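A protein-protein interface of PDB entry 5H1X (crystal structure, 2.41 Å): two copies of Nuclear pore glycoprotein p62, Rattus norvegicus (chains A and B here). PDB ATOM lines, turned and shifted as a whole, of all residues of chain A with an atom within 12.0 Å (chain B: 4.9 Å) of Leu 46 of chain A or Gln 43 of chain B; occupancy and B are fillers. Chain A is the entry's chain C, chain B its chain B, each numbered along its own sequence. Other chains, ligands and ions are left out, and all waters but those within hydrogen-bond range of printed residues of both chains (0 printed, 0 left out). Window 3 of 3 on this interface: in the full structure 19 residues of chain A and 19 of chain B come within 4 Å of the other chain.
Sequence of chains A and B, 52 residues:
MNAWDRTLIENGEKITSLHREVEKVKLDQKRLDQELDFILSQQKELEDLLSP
Among the printed residues, merely in contact across the chains: Glu 35 of chain A with Leu 40 of chain B, Ile 39 of chain A with Leu 40 of chain B, Gln 42 of chain A with Leu 40 of chain B, Gln 42 of chain A with Gln 43 of chain B, Leu 46 of chain A with Gln 43 of chain B, Leu 46 of chain A with Glu 47 of chain B and Leu 46 of chain A with Ser 51 of chain B.
The side-chain carboxylate (OE1) of Glu 47 of chain B sits close to the side-chain amide oxygen (OE1) of Gln 43 of chain B (2.5 Å). The backbone carbonyl oxygen (O) of Glu 47 of chain B sits at hydrogen-bond distance from the side-chain hydroxyl (OG) of Ser 51 of chain B. O of Ile 39 of chain A sits close to NE2 of Gln 42 of chain A (3.3 Å).
Printed residues of chain B within 4 Å of Ile 39 of chain A: Leu 40. Leu 46 of chain A touches just these residues of chain B: Gln 43, Glu 47 and Ser 51. Printed residues of chain A within 4 Å of Leu 40 of chain B: Glu 35, Ile 39 and Gln 42. Gln 42 of chain B touches none of the printed residues of chain A. No residue of chain A comes within 4 Å of Lys 44 of chain B. Of the printed residues of chain A, Glu 47 of chain B touches Leu 46 (3.4 Å). Of chain A, only Leu 46 comes within 4 Å of Ser 51 of chain B. The nearest residue of chain B that does not touch Leu 46 of chain A is Leu 50 of chain B (4.3 Å). The nearest residue of chain A that does not touch Gln 43 of chain B is Gln 43 of chain A (4.6 Å).
Of the 14 printed residues of chain A, 4 touch a printed residue of chain B. Hydrophobic or aromatic side chains of chain A within 4 Å of the printed part of chain B: Ile 39 and Leu 46. Among the printed residues, 7 pairs touch across the chains. Among the printed residues, no Asp or Glu carboxylate lies within 4 Å of a Lys or Arg side-chain nitrogen of the other chain.
Ile 39 of chain A touches Leu 40 of chain B, but with the chains exchanged Leu 40 of chain A does not touch Ile 39 of chain B (7.7 Å). Gln 42 of chain A touches Leu 40 of chain B, but with the chains exchanged Leu 40 of chain A does not touch Gln 42 of chain B (12.1 Å). Leu 46 of chain A touches Gln 43 of chain B, but with the chains exchanged Gln 43 of chain A does not touch Leu 46 of chain B (9.1 Å). Leu 46 of chain A touches Glu 47 of chain B, but with the chains exchanged Glu 47 of chain A does not touch Leu 46 of chain B (9.4 Å). Of the 7 pairs that touch across the chains among the printed residues, none has its exchanged pair printed and touching as well.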
ATOM      1  N   GLU A  35      -3.924  15.883   0.712  1.00  0.00           N
ATOM      2  CA  GLU A  35      -3.514  16.917   1.664  1.00  0.00           C
ATOM      3  C   GLU A  35      -2.622  16.336   2.745  1.00  0.00           C
ATOM      4  O   GLU A  35      -1.642  16.962   3.145  1.00  0.00           O
ATOM      5  CB  GLU A  35      -4.716  17.605   2.328  1.00  0.00           C
ATOM      6  CG  GLU A  35      -5.571  18.435   1.394  1.00  0.00           C
ATOM      7  CD  GLU A  35      -4.776  19.435   0.559  1.00  0.00           C
ATOM      8  OE1 GLU A  35      -3.743  19.973   1.036  1.00  0.00           O
ATOM      9  OE2 GLU A  35      -5.194  19.672  -0.597  1.00  0.00           O
ATOM     10  N   LEU A  36      -2.971  15.148   3.222  1.00  0.00           N
ATOM     11  CA  LEU A  36      -2.186  14.470   4.242  1.00  0.00           C
ATOM     12  C   LEU A  36      -0.776  14.161   3.787  1.00  0.00           C
ATOM     13  O   LEU A  36       0.188  14.400   4.532  1.00  0.00           O
ATOM     14  CB  LEU A  36      -2.859  13.179   4.659  1.00  0.00           C
ATOM     15  CG  LEU A  36      -3.852  13.388   5.787  1.00  0.00           C
ATOM     16  CD1 LEU A  36      -4.464  12.044   6.183  1.00  0.00           C
ATOM     17  CD2 LEU A  36      -3.109  14.054   6.938  1.00  0.00           C
ATOM     18  N   ASP A  37      -0.674  13.605   2.582  1.00  0.00           N
ATOM     19  CA  ASP A  37       0.613  13.322   1.955  1.00  0.00           C
ATOM     20  C   ASP A  37       1.481  14.583   1.981  1.00  0.00           C
ATOM     21  O   ASP A  37       2.627  14.564   2.434  1.00  0.00           O
ATOM     22  CB  ASP A  37       0.417  12.841   0.514  1.00  0.00           C
ATOM     23  CG  ASP A  37      -0.210  11.459   0.434  1.00  0.00           C
ATOM     24  OD1 ASP A  37      -0.117  10.685   1.413  1.00  0.00           O
ATOM     25  OD2 ASP A  37      -0.821  11.149  -0.613  1.00  0.00           O
ATOM     26  N   PHE A  38       0.905  15.689   1.526  1.00  0.00           N
ATOM     27  CA  PHE A  38       1.649  16.926   1.386  1.00  0.00           C
ATOM     28  C   PHE A  38       1.930  17.642   2.724  1.00  0.00           C
ATOM     29  O   PHE A  38       2.924  18.352   2.837  1.00  0.00           O
ATOM     30  CB  PHE A  38       0.911  17.852   0.417  1.00  0.00           C
ATOM     31  CG  PHE A  38       1.082  17.467  -1.041  1.00  0.00           C
ATOM     32  CD1 PHE A  38       0.328  16.448  -1.603  1.00  0.00           C
ATOM     33  CD2 PHE A  38       2.005  18.126  -1.846  1.00  0.00           C
ATOM     34  CE1 PHE A  38       0.477  16.094  -2.939  1.00  0.00           C
ATOM     35  CE2 PHE A  38       2.163  17.777  -3.191  1.00  0.00           C
ATOM     36  CZ  PHE A  38       1.392  16.761  -3.735  1.00  0.00           C
ATOM     37  N   ILE A  39       1.074  17.452   3.727  1.00  0.00           N
ATOM     38  CA  ILE A  39       1.322  17.988   5.066  1.00  0.00           C
ATOM     39  C   ILE A  39       2.455  17.220   5.732  1.00  0.00           C
ATOM     40  O   ILE A  39       3.299  17.799   6.425  1.00  0.00           O
ATOM     41  CB  ILE A  39       0.078  17.905   5.971  1.00  0.00           C
ATOM     42  CG1 ILE A  39      -0.978  18.930   5.551  1.00  0.00           C
ATOM     43  CG2 ILE A  39       0.451  18.134   7.424  1.00  0.00           C
ATOM     44  CD1 ILE A  39      -2.258  18.814   6.345  1.00  0.00           C
ATOM     45  N   LEU A  40       2.443  15.907   5.521  1.00  0.00           N
ATOM     46  CA  LEU A  40       3.527  15.016   5.919  1.00  0.00           C
ATOM     47  C   LEU A  40       4.879  15.527   5.399  1.00  0.00           C
ATOM     48  O   LEU A  40       5.756  15.926   6.170  1.00  0.00           O
ATOM     49  CB  LEU A  40       3.252  13.609   5.381  1.00  0.00           C
ATOM     50  CG  LEU A  40       4.119  12.441   5.842  1.00  0.00           C
ATOM     51  CD1 LEU A  40       4.375  12.540   7.338  1.00  0.00           C
ATOM     52  CD2 LEU A  40       3.457  11.118   5.488  1.00  0.00           C
ATOM     53  N   SER A  41       5.020  15.488   4.076  1.00  0.00           N
ATOM     54  CA  SER A  41       6.161  16.037   3.360  1.00  0.00           C
ATOM     55  C   SER A  41       6.533  17.446   3.843  1.00  0.00           C
ATOM     56  O   SER A  41       7.710  17.742   4.052  1.00  0.00           O
ATOM     57  CB  SER A  41       5.854  16.039   1.862  1.00  0.00           C
ATOM     58  OG  SER A  41       6.606  17.009   1.166  1.00  0.00           O
ATOM     59  N   GLN A  42       5.522  18.288   4.046  1.00  0.00           N
ATOM     60  CA  GLN A  42       5.708  19.660   4.519  1.00  0.00           C
ATOM     61  C   GLN A  42       6.515  19.771   5.828  1.00  0.00           C
ATOM     62  O   GLN A  42       7.462  20.564   5.906  1.00  0.00           O
ATOM     63  CB  GLN A  42       4.342  20.330   4.694  1.00  0.00           C
ATOM     64  CG  GLN A  42       4.231  21.293   5.881  1.00  0.00           C
ATOM     65  CD  GLN A  42       2.813  21.349   6.456  1.00  0.00           C
ATOM     66  OE1 GLN A  42       1.896  21.878   5.824  1.00  0.00           O
ATOM     67  NE2 GLN A  42       2.632  20.784   7.646  1.00  0.00           N
ATOM     68  N   GLN A  43       6.142  18.990   6.845  1.00  0.00           N
ATOM     69  CA  GLN A  43       6.851  19.020   8.120  1.00  0.00           C
ATOM     70  C   GLN A  43       8.260  18.472   7.962  1.00  0.00           C
ATOM     71  O   GLN A  43       9.200  18.951   8.618  1.00  0.00           O
ATOM     72  CB  GLN A  43       6.108  18.233   9.211  1.00  0.00           C
ATOM     73  CG  GLN A  43       4.607  18.478   9.263  1.00  0.00           C
ATOM     74  CD  GLN A  43       3.851  17.480  10.157  1.00  0.00           C
ATOM     75  OE1 GLN A  43       4.370  16.419  10.528  1.00  0.00           O
ATOM     76  NE2 GLN A  43       2.619  17.834  10.512  1.00  0.00           N
ATOM     77  N   LYS A  44       8.404  17.487   7.079  1.00  0.00           N
ATOM     78  CA  LYS A  44       9.679  16.808   6.922  1.00  0.00           C
ATOM     79  C   LYS A  44      10.735  17.710   6.276  1.00  0.00           C
ATOM     80  O   LYS A  44      11.904  17.690   6.676  1.00  0.00           O
ATOM     81  CB  LYS A  44       9.511  15.535   6.106  1.00  0.00           C
ATOM     82  CG  LYS A  44      10.457  14.435   6.523  1.00  0.00           C
ATOM     83  CD  LYS A  44      11.253  13.881   5.336  1.00  0.00           C
ATOM     84  CE  LYS A  44      10.518  14.037   4.015  1.00  0.00           C
ATOM     85  NZ  LYS A  44      11.444  14.174   2.851  1.00  0.00           N
ATOM     86  N   GLU A  45      10.335  18.506   5.287  1.00  0.00           N
ATOM     87  CA  GLU A  45      11.272  19.451   4.692  1.00  0.00           C
ATOM     88  C   GLU A  45      11.630  20.581   5.662  1.00  0.00           C
ATOM     89  O   GLU A  45      12.738  21.108   5.600  1.00  0.00           O
ATOM     90  CB  GLU A  45      10.727  20.030   3.384  1.00  0.00           C
ATOM     91  CG  GLU A  45      10.691  19.027   2.244  1.00  0.00           C
ATOM     92  CD  GLU A  45      10.100  19.609   0.967  1.00  0.00           C
ATOM     93  OE1 GLU A  45       9.646  20.778   1.000  1.00  0.00           O
ATOM     94  OE2 GLU A  45      10.065  18.883  -0.058  1.00  0.00           O
ATOM     95  N   LEU A  46      10.713  20.944   6.562  1.00  0.00           N
ATOM     96  CA  LEU A  46      11.012  21.957   7.577  1.00  0.00           C
ATOM     97  C   LEU A  46      12.100  21.450   8.504  1.00  0.00           C
ATOM     98  O   LEU A  46      12.885  22.227   9.048  1.00  0.00           O
ATOM     99  CB  LEU A  46       9.778  22.332   8.393  1.00  0.00           C
ATOM    100  CG  LEU A  46      10.058  23.391   9.470  1.00  0.00           C
ATOM    101  CD1 LEU A  46      10.760  24.609   8.860  1.00  0.00           C
ATOM    102  CD2 LEU A  46       8.796  23.803  10.224  1.00  0.00           C
ATOM    103  N   GLU A  47      12.136  20.138   8.687  1.00  0.00           N
ATOM    104  CA  GLU A  47      13.269  19.507   9.341  1.00  0.00           C
ATOM    105  C   GLU A  47      14.437  19.434   8.353  1.00  0.00           C
ATOM    106  O   GLU A  47      14.575  18.468   7.590  1.00  0.00           O
ATOM    107  CB  GLU A  47      12.881  18.127   9.874  1.00  0.00           C
ATOM    108  CG  GLU A  47      11.895  18.215  11.027  1.00  0.00           C
ATOM    109  CD  GLU A  47      10.748  17.243  10.905  1.00  0.00           C
ATOM    110  OE1 GLU A  47      10.931  16.181  10.275  1.00  0.00           O
ATOM    111  OE2 GLU A  47       9.659  17.550  11.434  1.00  0.00           O
ATOM    112  N   ASP A  48      15.257  20.486   8.372  1.00  0.00           N
ATOM    113  CA  ASP A  48      16.368  20.648   7.440  1.00  0.00           C
ATOM    114  C   ASP A  48      17.504  21.436   8.089  1.00  0.00           C
ATOM    115  O   ASP A  48      17.281  22.499   8.674  1.00  0.00           O
ATOM    116  CB  ASP A  48      15.904  21.359   6.167  1.00  0.00           C
ATOM    117  CG  ASP A  48      16.694  20.935   4.949  1.00  0.00           C
ATOM    118  OD1 ASP A  48      17.039  19.739   4.861  1.00  0.00           O
ATOM    119  OD2 ASP A  48      16.980  21.798   4.089  1.00  0.00           O
ATOM    120  N   ILE B  39      -4.245  23.489  10.150  1.00  0.00           N
ATOM    121  CA  ILE B  39      -2.877  22.984  10.167  1.00  0.00           C
ATOM    122  C   ILE B  39      -2.047  23.645   9.080  1.00  0.00           C
ATOM    123  O   ILE B  39      -0.889  24.038   9.293  1.00  0.00           O
ATOM    124  CB  ILE B  39      -2.837  21.477   9.973  1.00  0.00           C
ATOM    125  CG1 ILE B  39      -3.469  20.775  11.169  1.00  0.00           C
ATOM    126  CG2 ILE B  39      -1.410  21.002   9.788  1.00  0.00           C
ATOM    127  CD1 ILE B  39      -2.601  20.823  12.382  1.00  0.00           C
ATOM    128  N   LEU B  40      -2.662  23.787   7.914  1.00  0.00           N
ATOM    129  CA  LEU B  40      -1.983  24.394   6.787  1.00  0.00           C
ATOM    130  C   LEU B  40      -1.636  25.846   7.086  1.00  0.00           C
ATOM    131  O   LEU B  40      -0.548  26.301   6.748  1.00  0.00           O
ATOM    132  CB  LEU B  40      -2.837  24.273   5.522  1.00  0.00           C
ATOM    133  CG  LEU B  40      -2.810  22.836   4.972  1.00  0.00           C
ATOM    134  CD1 LEU B  40      -3.759  22.611   3.778  1.00  0.00           C
ATOM    135  CD2 LEU B  40      -1.370  22.406   4.632  1.00  0.00           C
ATOM    136  N   SER B  41      -2.558  26.558   7.733  1.00  0.00           N
ATOM    137  CA  SER B  41      -2.340  27.953   8.109  1.00  0.00           C
ATOM    138  C   SER B  41      -1.264  28.059   9.169  1.00  0.00           C
ATOM    139  O   SER B  41      -0.487  28.995   9.186  1.00  0.00           O
ATOM    140  CB  SER B  41      -3.631  28.583   8.636  1.00  0.00           C
ATOM    141  OG  SER B  41      -4.742  28.253   7.822  1.00  0.00           O
ATOM    142  N   GLN B  42      -1.248  27.075  10.056  1.00  0.00           N
ATOM    143  CA  GLN B  42      -0.343  27.040  11.184  1.00  0.00           C
ATOM    144  C   GLN B  42       1.091  26.761  10.754  1.00  0.00           C
ATOM    145  O   GLN B  42       2.020  27.360  11.279  1.00  0.00           O
ATOM    146  CB  GLN B  42      -0.821  25.982  12.167  1.00  0.00           C
ATOM    147  CG  GLN B  42       0.010  25.821  13.399  1.00  0.00           C
ATOM    148  CD  GLN B  42      -0.625  24.853  14.376  1.00  0.00           C
ATOM    149  OE1 GLN B  42      -1.065  23.752  13.998  1.00  0.00           O
ATOM    150  NE2 GLN B  42      -0.707  25.268  15.638  1.00  0.00           N
ATOM    151  N   GLN B  43       1.271  25.867   9.788  1.00  0.00           N
ATOM    152  CA  GLN B  43       2.610  25.514   9.320  1.00  0.00           C
ATOM    153  C   GLN B  43       3.147  26.536   8.336  1.00  0.00           C
ATOM    154  O   GLN B  43       4.339  26.602   8.127  1.00  0.00           O
ATOM    155  CB  GLN B  43       2.623  24.123   8.680  1.00  0.00           C
ATOM    156  CG  GLN B  43       3.402  23.087   9.499  1.00  0.00           C
ATOM    157  CD  GLN B  43       4.928  23.167   9.351  1.00  0.00           C
ATOM    158  OE1 GLN B  43       5.449  23.383   8.259  1.00  0.00           O
ATOM    159  NE2 GLN B  43       5.642  22.962  10.451  1.00  0.00           N
ATOM    160  N   LYS B  44       2.267  27.331   7.735  1.00  0.00           N
ATOM    161  CA  LYS B  44       2.692  28.462   6.915  1.00  0.00           C
ATOM    162  C   LYS B  44       3.373  29.547   7.757  1.00  0.00           C
ATOM    163  O   LYS B  44       4.409  30.079   7.370  1.00  0.00           O
ATOM    164  CB  LYS B  44       1.495  29.054   6.172  1.00  0.00           C
ATOM    165  CG  LYS B  44       1.617  30.540   5.862  1.00  0.00           C
ATOM    166  CD  LYS B  44       0.246  31.235   5.877  1.00  0.00           C
ATOM    167  CE  LYS B  44      -0.115  31.773   7.266  1.00  0.00           C
ATOM    168  NZ  LYS B  44       0.656  33.033   7.548  1.00  0.00           N
ATOM    169  N   GLU B  45       2.774  29.870   8.904  1.00  0.00           N
ATOM    170  CA  GLU B  45       3.326  30.854   9.838  1.00  0.00           C
ATOM    171  C   GLU B  45       4.621  30.379  10.457  1.00  0.00           C
ATOM    172  O   GLU B  45       5.524  31.167  10.690  1.00  0.00           O
ATOM    173  CB  GLU B  45       2.328  31.156  10.965  1.00  0.00           C
ATOM    174  CG  GLU B  45       1.163  32.024  10.564  1.00  0.00           C
ATOM    175  CD  GLU B  45       1.528  33.492  10.527  1.00  0.00           C
ATOM    176  OE1 GLU B  45       1.898  34.043  11.594  1.00  0.00           O
ATOM    177  OE2 GLU B  45       1.464  34.090   9.430  1.00  0.00           O
ATOM    178  N   LEU B  46       4.705  29.083  10.724  1.00  0.00           N
ATOM    179  CA  LEU B  46       5.798  28.555  11.520  1.00  0.00           C
ATOM    180  C   LEU B  46       7.105  28.341  10.735  1.00  0.00           C
ATOM    181  O   LEU B  46       8.178  28.300  11.330  1.00  0.00           O
ATOM    182  CB  LEU B  46       5.354  27.257  12.197  1.00  0.00           C
ATOM    183  CG  LEU B  46       4.766  27.433  13.609  1.00  0.00           C
ATOM    184  CD1 LEU B  46       3.939  28.704  13.737  1.00  0.00           C
ATOM    185  CD2 LEU B  46       3.920  26.229  14.009  1.00  0.00           C
ATOM    186  N   GLU B  47       7.047  28.213   9.413  1.00  0.00           N
ATOM    187  CA  GLU B  47       8.306  28.185   8.674  1.00  0.00           C
ATOM    188  C   GLU B  47       8.593  29.529   8.025  1.00  0.00           C
ATOM    189  O   GLU B  47       9.734  29.803   7.663  1.00  0.00           O
ATOM    190  CB  GLU B  47       8.334  27.075   7.622  1.00  0.00           C
ATOM    191  CG  GLU B  47       7.020  26.754   6.984  1.00  0.00           C
ATOM    192  CD  GLU B  47       6.993  25.360   6.372  1.00  0.00           C
ATOM    193  OE1 GLU B  47       7.434  24.402   7.045  1.00  0.00           O
ATOM    194  OE2 GLU B  47       6.514  25.219   5.226  1.00  0.00           O
ATOM    195  N   LEU B  50      11.019  30.951  10.692  1.00  0.00           N
ATOM    196  CA  LEU B  50      12.442  30.644  10.444  1.00  0.00           C
ATOM    197  C   LEU B  50      12.700  29.656   9.311  1.00  0.00           C
ATOM    198  O   LEU B  50      12.623  28.456   9.525  1.00  0.00           O
ATOM    199  CB  LEU B  50      13.141  30.072  11.689  1.00  0.00           C
ATOM    200  CG  LEU B  50      14.647  30.023  11.362  1.00  0.00           C
ATOM    201  CD1 LEU B  50      15.195  31.371  10.886  1.00  0.00           C
ATOM    202  CD2 LEU B  50      15.521  29.362  12.394  1.00  0.00           C
ATOM    203  N   SER B  51      13.083  30.160   8.143  1.00  0.00           N
ATOM    204  CA  SER B  51      13.539  29.322   7.044  1.00  0.00           C
ATOM    205  C   SER B  51      14.110  30.216   5.953  1.00  0.00           C
ATOM    206  O   SER B  51      13.589  31.300   5.700  1.00  0.00           O
ATOM    207  CB  SER B  51      12.398  28.451   6.482  1.00  0.00           C
ATOM    208  OG  SER B  51      11.848  27.576   7.463  1.00  0.00           O
